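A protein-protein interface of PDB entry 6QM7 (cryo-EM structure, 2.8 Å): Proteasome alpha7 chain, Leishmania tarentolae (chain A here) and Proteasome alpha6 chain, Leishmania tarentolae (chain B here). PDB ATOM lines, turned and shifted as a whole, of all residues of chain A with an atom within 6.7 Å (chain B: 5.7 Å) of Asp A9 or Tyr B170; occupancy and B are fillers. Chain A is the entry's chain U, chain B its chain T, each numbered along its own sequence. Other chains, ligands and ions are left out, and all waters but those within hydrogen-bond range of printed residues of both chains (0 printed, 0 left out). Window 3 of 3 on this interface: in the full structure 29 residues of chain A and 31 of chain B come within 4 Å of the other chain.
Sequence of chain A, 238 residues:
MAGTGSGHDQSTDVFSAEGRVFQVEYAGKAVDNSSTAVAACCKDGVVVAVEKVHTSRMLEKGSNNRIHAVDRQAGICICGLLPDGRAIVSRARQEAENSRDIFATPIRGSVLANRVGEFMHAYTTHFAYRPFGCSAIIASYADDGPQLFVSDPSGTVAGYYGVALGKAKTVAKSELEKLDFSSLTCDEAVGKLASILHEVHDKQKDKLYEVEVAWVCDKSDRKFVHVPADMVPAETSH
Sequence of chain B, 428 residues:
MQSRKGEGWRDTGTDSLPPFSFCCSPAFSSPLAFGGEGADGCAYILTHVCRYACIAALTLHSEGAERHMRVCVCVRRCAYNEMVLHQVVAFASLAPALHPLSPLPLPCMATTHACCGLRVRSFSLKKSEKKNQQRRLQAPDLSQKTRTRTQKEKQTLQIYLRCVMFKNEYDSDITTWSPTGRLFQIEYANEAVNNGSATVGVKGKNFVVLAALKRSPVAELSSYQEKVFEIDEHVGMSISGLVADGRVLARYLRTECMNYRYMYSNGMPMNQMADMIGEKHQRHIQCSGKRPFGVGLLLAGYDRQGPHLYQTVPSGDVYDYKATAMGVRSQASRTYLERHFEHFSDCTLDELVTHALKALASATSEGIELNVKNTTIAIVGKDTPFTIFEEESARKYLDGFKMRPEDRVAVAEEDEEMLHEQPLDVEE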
ATOM      1  N   SER A   6     -10.680  23.172  -6.820  1.00  0.00           N
ATOM      2  CA  SER A   6     -10.719  22.219  -5.657  1.00  0.00           C
ATOM      3  C   SER A   6      -9.656  22.587  -4.607  1.00  0.00           C
ATOM      4  O   SER A   6      -9.978  22.505  -3.405  1.00  0.00           O
ATOM      5  CB  SER A   6     -10.570  20.781  -6.116  1.00  0.00           C
ATOM      6  OG  SER A   6      -9.414  20.613  -6.924  1.00  0.00           O
ATOM      7  N   GLY A   7      -8.448  22.972  -5.041  1.00  0.00           N
ATOM      8  CA  GLY A   7      -7.296  23.287  -4.170  1.00  0.00           C
ATOM      9  C   GLY A   7      -7.340  24.699  -3.602  1.00  0.00           C
ATOM     10  O   GLY A   7      -6.565  24.969  -2.659  1.00  0.00           O
ATOM     11  N   HIS A   8      -8.202  25.568  -4.145  1.00  0.00           N
ATOM     12  CA  HIS A   8      -8.336  27.003  -3.758  1.00  0.00           C
ATOM     13  C   HIS A   8      -8.769  27.166  -2.292  1.00  0.00           C
ATOM     14  O   HIS A   8      -8.465  28.239  -1.744  1.00  0.00           O
ATOM     15  CB  HIS A   8      -9.248  27.772  -4.740  1.00  0.00           C
ATOM     16  CG  HIS A   8     -10.686  27.355  -4.778  1.00  0.00           C
ATOM     17  ND1 HIS A   8     -11.083  26.031  -4.913  1.00  0.00           N
ATOM     18  CD2 HIS A   8     -11.825  28.085  -4.757  1.00  0.00           C
ATOM     19  CE1 HIS A   8     -12.401  25.962  -4.939  1.00  0.00           C
ATOM     20  NE2 HIS A   8     -12.881  27.211  -4.841  1.00  0.00           N
ATOM     21  N   ASP A   9      -9.416  26.162  -1.675  1.00  0.00           N
ATOM     22  CA  ASP A   9     -10.150  26.301  -0.385  1.00  0.00           C
ATOM     23  C   ASP A   9      -9.742  25.250   0.658  1.00  0.00           C
ATOM     24  O   ASP A   9     -10.456  25.135   1.675  1.00  0.00           O
ATOM     25  CB  ASP A   9     -11.656  26.227  -0.639  1.00  0.00           C
ATOM     26  CG  ASP A   9     -12.176  24.843  -0.987  1.00  0.00           C
ATOM     27  OD1 ASP A   9     -13.420  24.690  -1.043  1.00  0.00           O
ATOM     28  OD2 ASP A   9     -11.341  23.928  -1.189  1.00  0.00           O
ATOM     29  N   GLN A  10      -8.660  24.506   0.434  1.00  0.00           N
ATOM     30  CA  GLN A  10      -8.276  23.359   1.301  1.00  0.00           C
ATOM     31  C   GLN A  10      -7.586  23.866   2.564  1.00  0.00           C
ATOM     32  O   GLN A  10      -7.697  23.183   3.604  1.00  0.00           O
ATOM     33  CB  GLN A  10      -7.362  22.372   0.571  1.00  0.00           C
ATOM     34  CG  GLN A  10      -8.089  21.514  -0.454  1.00  0.00           C
ATOM     35  CD  GLN A  10      -9.201  20.707   0.166  1.00  0.00           C
ATOM     36  OE1 GLN A  10      -9.024  20.074   1.204  1.00  0.00           O
ATOM     37  NE2 GLN A  10     -10.364  20.749  -0.464  1.00  0.00           N
ATOM     38  N   SER A  11      -6.872  24.986   2.469  1.00  0.00           N
ATOM     39  CA  SER A  11      -6.158  25.587   3.618  1.00  0.00           C
ATOM     40  C   SER A  11      -6.302  27.104   3.602  1.00  0.00           C
ATOM     41  O   SER A  11      -6.598  27.699   2.554  1.00  0.00           O
ATOM     42  CB  SER A  11      -4.715  25.172   3.659  1.00  0.00           C
ATOM     43  OG  SER A  11      -3.953  25.948   2.749  1.00  0.00           O
ATOM     44  N   THR A  12      -6.087  27.679   4.771  1.00  0.00           N
ATOM     45  CA  THR A  12      -6.295  29.108   5.052  1.00  0.00           C
ATOM     46  C   THR A  12      -5.072  29.899   4.594  1.00  0.00           C
ATOM     47  O   THR A  12      -5.157  31.128   4.620  1.00  0.00           O
ATOM     48  CB  THR A  12      -6.589  29.307   6.538  1.00  0.00           C
ATOM     49  OG1 THR A  12      -7.151  30.612   6.692  1.00  0.00           O
ATOM     50  CG2 THR A  12      -5.359  29.146   7.407  1.00  0.00           C
ATOM     51  N   VAL A  14      -4.102  30.187   1.686  1.00  0.00           N
ATOM     52  CA  VAL A  14      -4.315  30.324   0.224  1.00  0.00           C
ATOM     53  C   VAL A  14      -5.438  31.323  -0.003  1.00  0.00           C
ATOM     54  O   VAL A  14      -6.578  31.012   0.384  1.00  0.00           O
ATOM     55  CB  VAL A  14      -4.669  28.969  -0.414  1.00  0.00           C
ATOM     56  CG1 VAL A  14      -4.895  29.108  -1.913  1.00  0.00           C
ATOM     57  CG2 VAL A  14      -3.610  27.919  -0.114  1.00  0.00           C
ATOM     58  N   SER A  16      -8.023  32.780  -2.773  1.00  0.00           N
ATOM     59  CA  SER A  16      -8.699  32.464  -4.060  1.00  0.00           C
ATOM     60  C   SER A  16      -8.374  33.572  -5.057  1.00  0.00           C
ATOM     61  O   SER A  16      -7.792  34.587  -4.633  1.00  0.00           O
ATOM     62  CB  SER A  16     -10.188  32.333  -3.898  1.00  0.00           C
ATOM     63  OG  SER A  16     -10.823  33.608  -3.895  1.00  0.00           O
ATOM     64  N   VAL A  21     -10.372  34.131   1.446  1.00  0.00           N
ATOM     65  CA  VAL A  21      -9.713  33.019   2.178  1.00  0.00           C
ATOM     66  C   VAL A  21     -10.812  32.065   2.617  1.00  0.00           C
ATOM     67  O   VAL A  21     -11.272  32.177   3.750  1.00  0.00           O
ATOM     68  CB  VAL A  21      -8.901  33.556   3.373  1.00  0.00           C
ATOM     69  CG1 VAL A  21      -8.087  32.460   4.040  1.00  0.00           C
ATOM     70  CG2 VAL A  21      -8.016  34.734   2.982  1.00  0.00           C
ATOM     71  N   PHE A  22     -11.212  31.170   1.723  1.00  0.00           N
ATOM     72  CA  PHE A  22     -12.413  30.315   1.861  1.00  0.00           C
ATOM     73  C   PHE A  22     -12.433  29.567   3.199  1.00  0.00           C
ATOM     74  O   PHE A  22     -13.507  29.476   3.794  1.00  0.00           O
ATOM     75  CB  PHE A  22     -12.509  29.357   0.681  1.00  0.00           C
ATOM     76  CG  PHE A  22     -13.159  29.973  -0.525  1.00  0.00           C
ATOM     77  CD1 PHE A  22     -14.512  30.282  -0.509  1.00  0.00           C
ATOM     78  CD2 PHE A  22     -12.434  30.241  -1.671  1.00  0.00           C
ATOM     79  CE1 PHE A  22     -15.131  30.843  -1.616  1.00  0.00           C
ATOM     80  CE2 PHE A  22     -13.057  30.798  -2.779  1.00  0.00           C
ATOM     81  CZ  PHE A  22     -14.399  31.097  -2.751  1.00  0.00           C
ATOM     82  N   GLN A  23     -11.312  29.048   3.679  1.00  0.00           N
ATOM     83  CA  GLN A  23     -11.320  28.300   4.962  1.00  0.00           C
ATOM     84  C   GLN A  23     -11.813  29.181   6.112  1.00  0.00           C
ATOM     85  O   GLN A  23     -12.445  28.624   7.029  1.00  0.00           O
ATOM     86  CB  GLN A  23      -9.937  27.751   5.290  1.00  0.00           C
ATOM     87  CG  GLN A  23      -9.651  26.440   4.586  1.00  0.00           C
ATOM     88  CD  GLN A  23     -10.459  25.324   5.188  1.00  0.00           C
ATOM     89  OE1 GLN A  23     -10.248  24.967   6.337  1.00  0.00           O
ATOM     90  NE2 GLN A  23     -11.389  24.776   4.422  1.00  0.00           N
ATOM     91  N   TYR A  26     -15.583  29.513   5.768  1.00  0.00           N
ATOM     92  CA  TYR A  26     -16.158  28.201   6.136  1.00  0.00           C
ATOM     93  C   TYR A  26     -16.187  28.068   7.660  1.00  0.00           C
ATOM     94  O   TYR A  26     -17.162  27.528   8.203  1.00  0.00           O
ATOM     95  CB  TYR A  26     -15.331  27.080   5.507  1.00  0.00           C
ATOM     96  CG  TYR A  26     -15.349  27.000   4.003  1.00  0.00           C
ATOM     97  CD1 TYR A  26     -16.200  27.783   3.238  1.00  0.00           C
ATOM     98  CD2 TYR A  26     -14.542  26.087   3.337  1.00  0.00           C
ATOM     99  CE1 TYR A  26     -16.229  27.684   1.856  1.00  0.00           C
ATOM    100  CE2 TYR A  26     -14.564  25.972   1.952  1.00  0.00           C
ATOM    101  CZ  TYR A  26     -15.415  26.774   1.208  1.00  0.00           C
ATOM    102  OH  TYR A  26     -15.463  26.707  -0.152  1.00  0.00           O
ATOM    103  N   ASN B 168     -15.448  13.074  -1.068  1.00  0.00           N
ATOM    104  CA  ASN B 168     -15.368  14.214  -0.094  1.00  0.00           C
ATOM    105  C   ASN B 168     -13.913  14.698  -0.037  1.00  0.00           C
ATOM    106  O   ASN B 168     -13.058  13.923   0.435  1.00  0.00           O
ATOM    107  CB  ASN B 168     -15.894  13.806   1.289  1.00  0.00           C
ATOM    108  CG  ASN B 168     -16.293  14.977   2.163  1.00  0.00           C
ATOM    109  OD1 ASN B 168     -15.819  16.097   1.979  1.00  0.00           O
ATOM    110  ND2 ASN B 168     -17.165  14.724   3.128  1.00  0.00           N
ATOM    111  N   GLU B 169     -13.645  15.926  -0.498  1.00  0.00           N
ATOM    112  CA  GLU B 169     -12.263  16.488  -0.589  1.00  0.00           C
ATOM    113  C   GLU B 169     -11.883  17.187   0.728  1.00  0.00           C
ATOM    114  O   GLU B 169     -10.732  17.663   0.814  1.00  0.00           O
ATOM    115  CB  GLU B 169     -12.054  17.417  -1.800  1.00  0.00           C
ATOM    116  CG  GLU B 169     -13.261  18.234  -2.257  1.00  0.00           C
ATOM    117  CD  GLU B 169     -14.039  17.666  -3.437  1.00  0.00           C
ATOM    118  OE1 GLU B 169     -14.582  18.472  -4.225  1.00  0.00           O
ATOM    119  OE2 GLU B 169     -14.100  16.424  -3.574  1.00  0.00           O
ATOM    120  N   TYR B 170     -12.773  17.197   1.729  1.00  0.00           N
ATOM    121  CA  TYR B 170     -12.648  18.007   2.968  1.00  0.00           C
ATOM    122  C   TYR B 170     -12.488  17.136   4.222  1.00  0.00           C
ATOM    123  O   TYR B 170     -12.361  17.730   5.317  1.00  0.00           O
ATOM    124  CB  TYR B 170     -13.878  18.902   3.106  1.00  0.00           C
ATOM    125  CG  TYR B 170     -14.066  19.857   1.956  1.00  0.00           C
ATOM    126  CD1 TYR B 170     -13.191  20.915   1.757  1.00  0.00           C
ATOM    127  CD2 TYR B 170     -15.109  19.695   1.056  1.00  0.00           C
ATOM    128  CE1 TYR B 170     -13.351  21.795   0.698  1.00  0.00           C
ATOM    129  CE2 TYR B 170     -15.281  20.565  -0.010  1.00  0.00           C
ATOM    130  CZ  TYR B 170     -14.401  21.619  -0.187  1.00  0.00           C
ATOM    131  OH  TYR B 170     -14.575  22.477  -1.233  1.00  0.00           O
ATOM    132  N   ASP B 171     -12.469  15.803   4.093  1.00  0.00           N
ATOM    133  CA  ASP B 171     -12.527  14.862   5.248  1.00  0.00           C
ATOM    134  C   ASP B 171     -11.140  14.288   5.587  1.00  0.00           C
ATOM    135  O   ASP B 171     -11.062  13.496   6.539  1.00  0.00           O
ATOM    136  CB  ASP B 171     -13.585  13.787   4.992  1.00  0.00           C
ATOM    137  CG  ASP B 171     -13.155  12.625   4.109  1.00  0.00           C
ATOM    138  OD1 ASP B 171     -12.191  12.794   3.333  1.00  0.00           O
ATOM    139  OD2 ASP B 171     -13.802  11.555   4.195  1.00  0.00           O
ATOM    140  N   SER B 172     -10.087  14.694   4.871  1.00  0.00           N
ATOM    141  CA  SER B 172      -8.730  14.092   4.939  1.00  0.00           C
ATOM    142  C   SER B 172      -7.964  14.678   6.130  1.00  0.00           C
ATOM    143  O   SER B 172      -7.458  13.887   6.940  1.00  0.00           O
ATOM    144  CB  SER B 172      -7.956  14.288   3.643  1.00  0.00           C
ATOM    145  OG  SER B 172      -8.820  14.544   2.544  1.00  0.00           O
ATOM    146  N   ASP B 173      -7.867  16.008   6.213  1.00  0.00           N
ATOM    147  CA  ASP B 173      -7.050  16.736   7.223  1.00  0.00           C
ATOM    148  C   ASP B 173      -7.968  17.289   8.323  1.00  0.00           C
ATOM    149  O   ASP B 173      -9.148  17.599   8.050  1.00  0.00           O
ATOM    150  CB  ASP B 173      -6.197  17.828   6.556  1.00  0.00           C
ATOM    151  CG  ASP B 173      -4.823  18.083   7.189  1.00  0.00           C
ATOM    152  OD1 ASP B 173      -4.717  18.048   8.442  1.00  0.00           O
ATOM    153  OD2 ASP B 173      -3.853  18.322   6.423  1.00  0.00           O
ATOM    154  N   THR B 176      -8.897  21.192   7.841  1.00  0.00           N
ATOM    155  CA  THR B 176      -9.806  21.570   6.744  1.00  0.00           C
ATOM    156  C   THR B 176     -11.238  21.657   7.255  1.00  0.00           C
ATOM    157  O   THR B 176     -11.826  20.612   7.559  1.00  0.00           O
ATOM    158  CB  THR B 176      -9.673  20.613   5.567  1.00  0.00           C
ATOM    159  OG1 THR B 176      -8.283  20.574   5.244  1.00  0.00           O
ATOM    160  CG2 THR B 176     -10.497  21.072   4.386  1.00  0.00           C
ATOM    161  N   TRP B 177     -11.771  22.872   7.328  1.00  0.00           N
ATOM    162  CA  TRP B 177     -13.228  23.127   7.359  1.00  0.00           C
ATOM    163  C   TRP B 177     -13.827  22.651   6.045  1.00  0.00           C
ATOM    164  O   TRP B 177     -13.231  22.939   5.000  1.00  0.00           O
ATOM    165  CB  TRP B 177     -13.508  24.613   7.546  1.00  0.00           C
ATOM    166  CG  TRP B 177     -13.136  25.099   8.903  1.00  0.00           C
ATOM    167  CD1 TRP B 177     -11.963  25.673   9.293  1.00  0.00           C
ATOM    168  CD2 TRP B 177     -13.942  24.994  10.080  1.00  0.00           C
ATOM    169  NE1 TRP B 177     -11.988  25.946  10.629  1.00  0.00           N
ATOM    170  CE2 TRP B 177     -13.195  25.553  11.138  1.00  0.00           C
ATOM    171  CE3 TRP B 177     -15.221  24.491  10.330  1.00  0.00           C
ATOM    172  CZ2 TRP B 177     -13.699  25.630  12.434  1.00  0.00           C
ATOM    173  CZ3 TRP B 177     -15.719  24.573  11.606  1.00  0.00           C
ATOM    174  CH2 TRP B 177     -14.965  25.127  12.641  1.00  0.00           C
ATOM    175  N   SER B 178     -14.983  21.993   6.097  1.00  0.00           N
ATOM    176  CA  SER B 178     -15.869  21.802   4.921  1.00  0.00           C
ATOM    177  C   SER B 178     -16.494  23.147   4.582  1.00  0.00           C
ATOM    178  O   SER B 178     -16.484  24.040   5.420  1.00  0.00           O
ATOM    179  CB  SER B 178     -16.935  20.752   5.160  1.00  0.00           C
ATOM    180  OG  SER B 178     -18.073  21.295   5.820  1.00  0.00           O
ATOM    181  N   PRO B 179     -17.101  23.313   3.387  1.00  0.00           N
ATOM    182  CA  PRO B 179     -17.845  24.529   3.045  1.00  0.00           C
ATOM    183  C   PRO B 179     -19.110  24.763   3.881  1.00  0.00           C
ATOM    184  O   PRO B 179     -19.529  25.889   3.960  1.00  0.00           O
ATOM    185  CB  PRO B 179     -18.248  24.324   1.584  1.00  0.00           C
ATOM    186  CG  PRO B 179     -17.273  23.286   1.096  1.00  0.00           C
ATOM    187  CD  PRO B 179     -17.082  22.361   2.276  1.00  0.00           C
ATOM    188  N   PHE B 184     -14.716  17.312   9.597  1.00  0.00           N
ATOM    189  CA  PHE B 184     -15.074  15.891   9.386  1.00  0.00           C
ATOM    190  C   PHE B 184     -14.160  14.978  10.200  1.00  0.00           C
ATOM    191  O   PHE B 184     -14.666  14.017  10.778  1.00  0.00           O
ATOM    192  CB  PHE B 184     -15.033  15.545   7.904  1.00  0.00           C
ATOM    193  CG  PHE B 184     -16.295  15.895   7.166  1.00  0.00           C
ATOM    194  CD1 PHE B 184     -17.433  15.121   7.316  1.00  0.00           C
ATOM    195  CD2 PHE B 184     -16.342  16.981   6.311  1.00  0.00           C
ATOM    196  CE1 PHE B 184     -18.592  15.427   6.621  1.00  0.00           C
ATOM    197  CE2 PHE B 184     -17.500  17.282   5.611  1.00  0.00           C
ATOM    198  CZ  PHE B 184     -18.624  16.506   5.767  1.00  0.00           C
ATOM    199  N   GLN B 185     -12.866  15.261  10.275  1.00  0.00           N
ATOM    200  CA  GLN B 185     -11.938  14.402  11.054  1.00  0.00           C
ATOM    201  C   GLN B 185     -12.405  14.311  12.509  1.00  0.00           C
ATOM    202  O   GLN B 185     -12.133  13.269  13.135  1.00  0.00           O
ATOM    203  CB  GLN B 185     -10.487  14.874  10.955  1.00  0.00           C
ATOM    204  CG  GLN B 185      -9.774  14.341   9.717  1.00  0.00           C
ATOM    205  CD  GLN B 185      -9.656  12.839   9.726  1.00  0.00           C
ATOM    206  OE1 GLN B 185      -8.906  12.275  10.513  1.00  0.00           O
ATOM    207  NE2 GLN B 185     -10.416  12.185   8.862  1.00  0.00           N
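Hydrophobic or aromatic side chains of chain B that line the printed part of chain A: Tyr B170, Trp B177 and Pro B179. Of the 13 printed residues of chain A, 4 touch a printed residue of chain B. Hydrophobic or aromatic side chains of chain A within 4 Å of the printed part of chain B: Tyr A26. Among the printed residues, no Asp or Glu carboxylate lies within 4 Å of a Lys or Arg side-chain nitrogen of the other chain.
Among the printed residues, pairs that only touch across the chains: Tyr A26 with Ser B178 (3.3 Å), Gln A10 with Tyr B170 (3.4 Å), Gln A23 with Thr B176 (3.4 Å), Tyr A26 with Pro B179 (3.6 Å) and Tyr A26 with Trp B177 (3.7 Å).
The side-chain amide oxygen of Asn B168 lies within hydrogen-bond range of the backbone NH of Tyr B170 (3.2 Å). O of Ser A6 is in hydrogen-bond range of NE2 of Gln A10. OD2 of Asp A9 sits at hydrogen-bond distance from NE2 of Gln A10 (3.4 Å). The backbone carbonyl oxygen of Asp A9 is in hydrogen-bond range of the side-chain amide nitrogen of Gln A23, at 2.9 Å. The side-chain carboxylate (OD1) of Asp A9 is in hydrogen-bond range of the side-chain hydroxyl (OH) of Tyr A26 (3.0 Å).
OE1 of Gln A10 lies close to O of Glu B169 (3.0 Å). The side-chain carboxylate (OD1) of Asp A9 sits at hydrogen-bond distance from the side-chain hydroxyl (OH) of Tyr B170 (2.5 Å). The side-chain hydroxyl (OG1) of Thr B176 lies within hydrogen-bond range of the backbone carbonyl oxygen (O) of Gln A10 (3.1 Å). The backbone carbonyl oxygen (O) of Trp B177 sits at hydrogen-bond distance from the side-chain amide nitrogen (NE2) of Gln A23.
Gly A7 touches none of the printed residues of chain B. Of the printed residues of chain A, Glu B169 touches Gln A10. Of the printed residues of chain A, Thr B176 touches Gln A10 (3.1 Å) and Gln A23 (3.4 Å). Of the printed residues of chain A, Ser B178 touches Tyr A26 (3.3 Å). Of the printed residues of chain A, Pro B179 touches Tyr A26 (3.6 Å). The nearest residue of chain B that does not touch Asp A9 is Pro B179 (4.6 Å). The nearest residue of chain A that does not touch Tyr B170 is Tyr A26 (4.5 Å). The nearest printed residue of chain A that does not touch Ser B178 is Gln A23 (4.8 Å).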
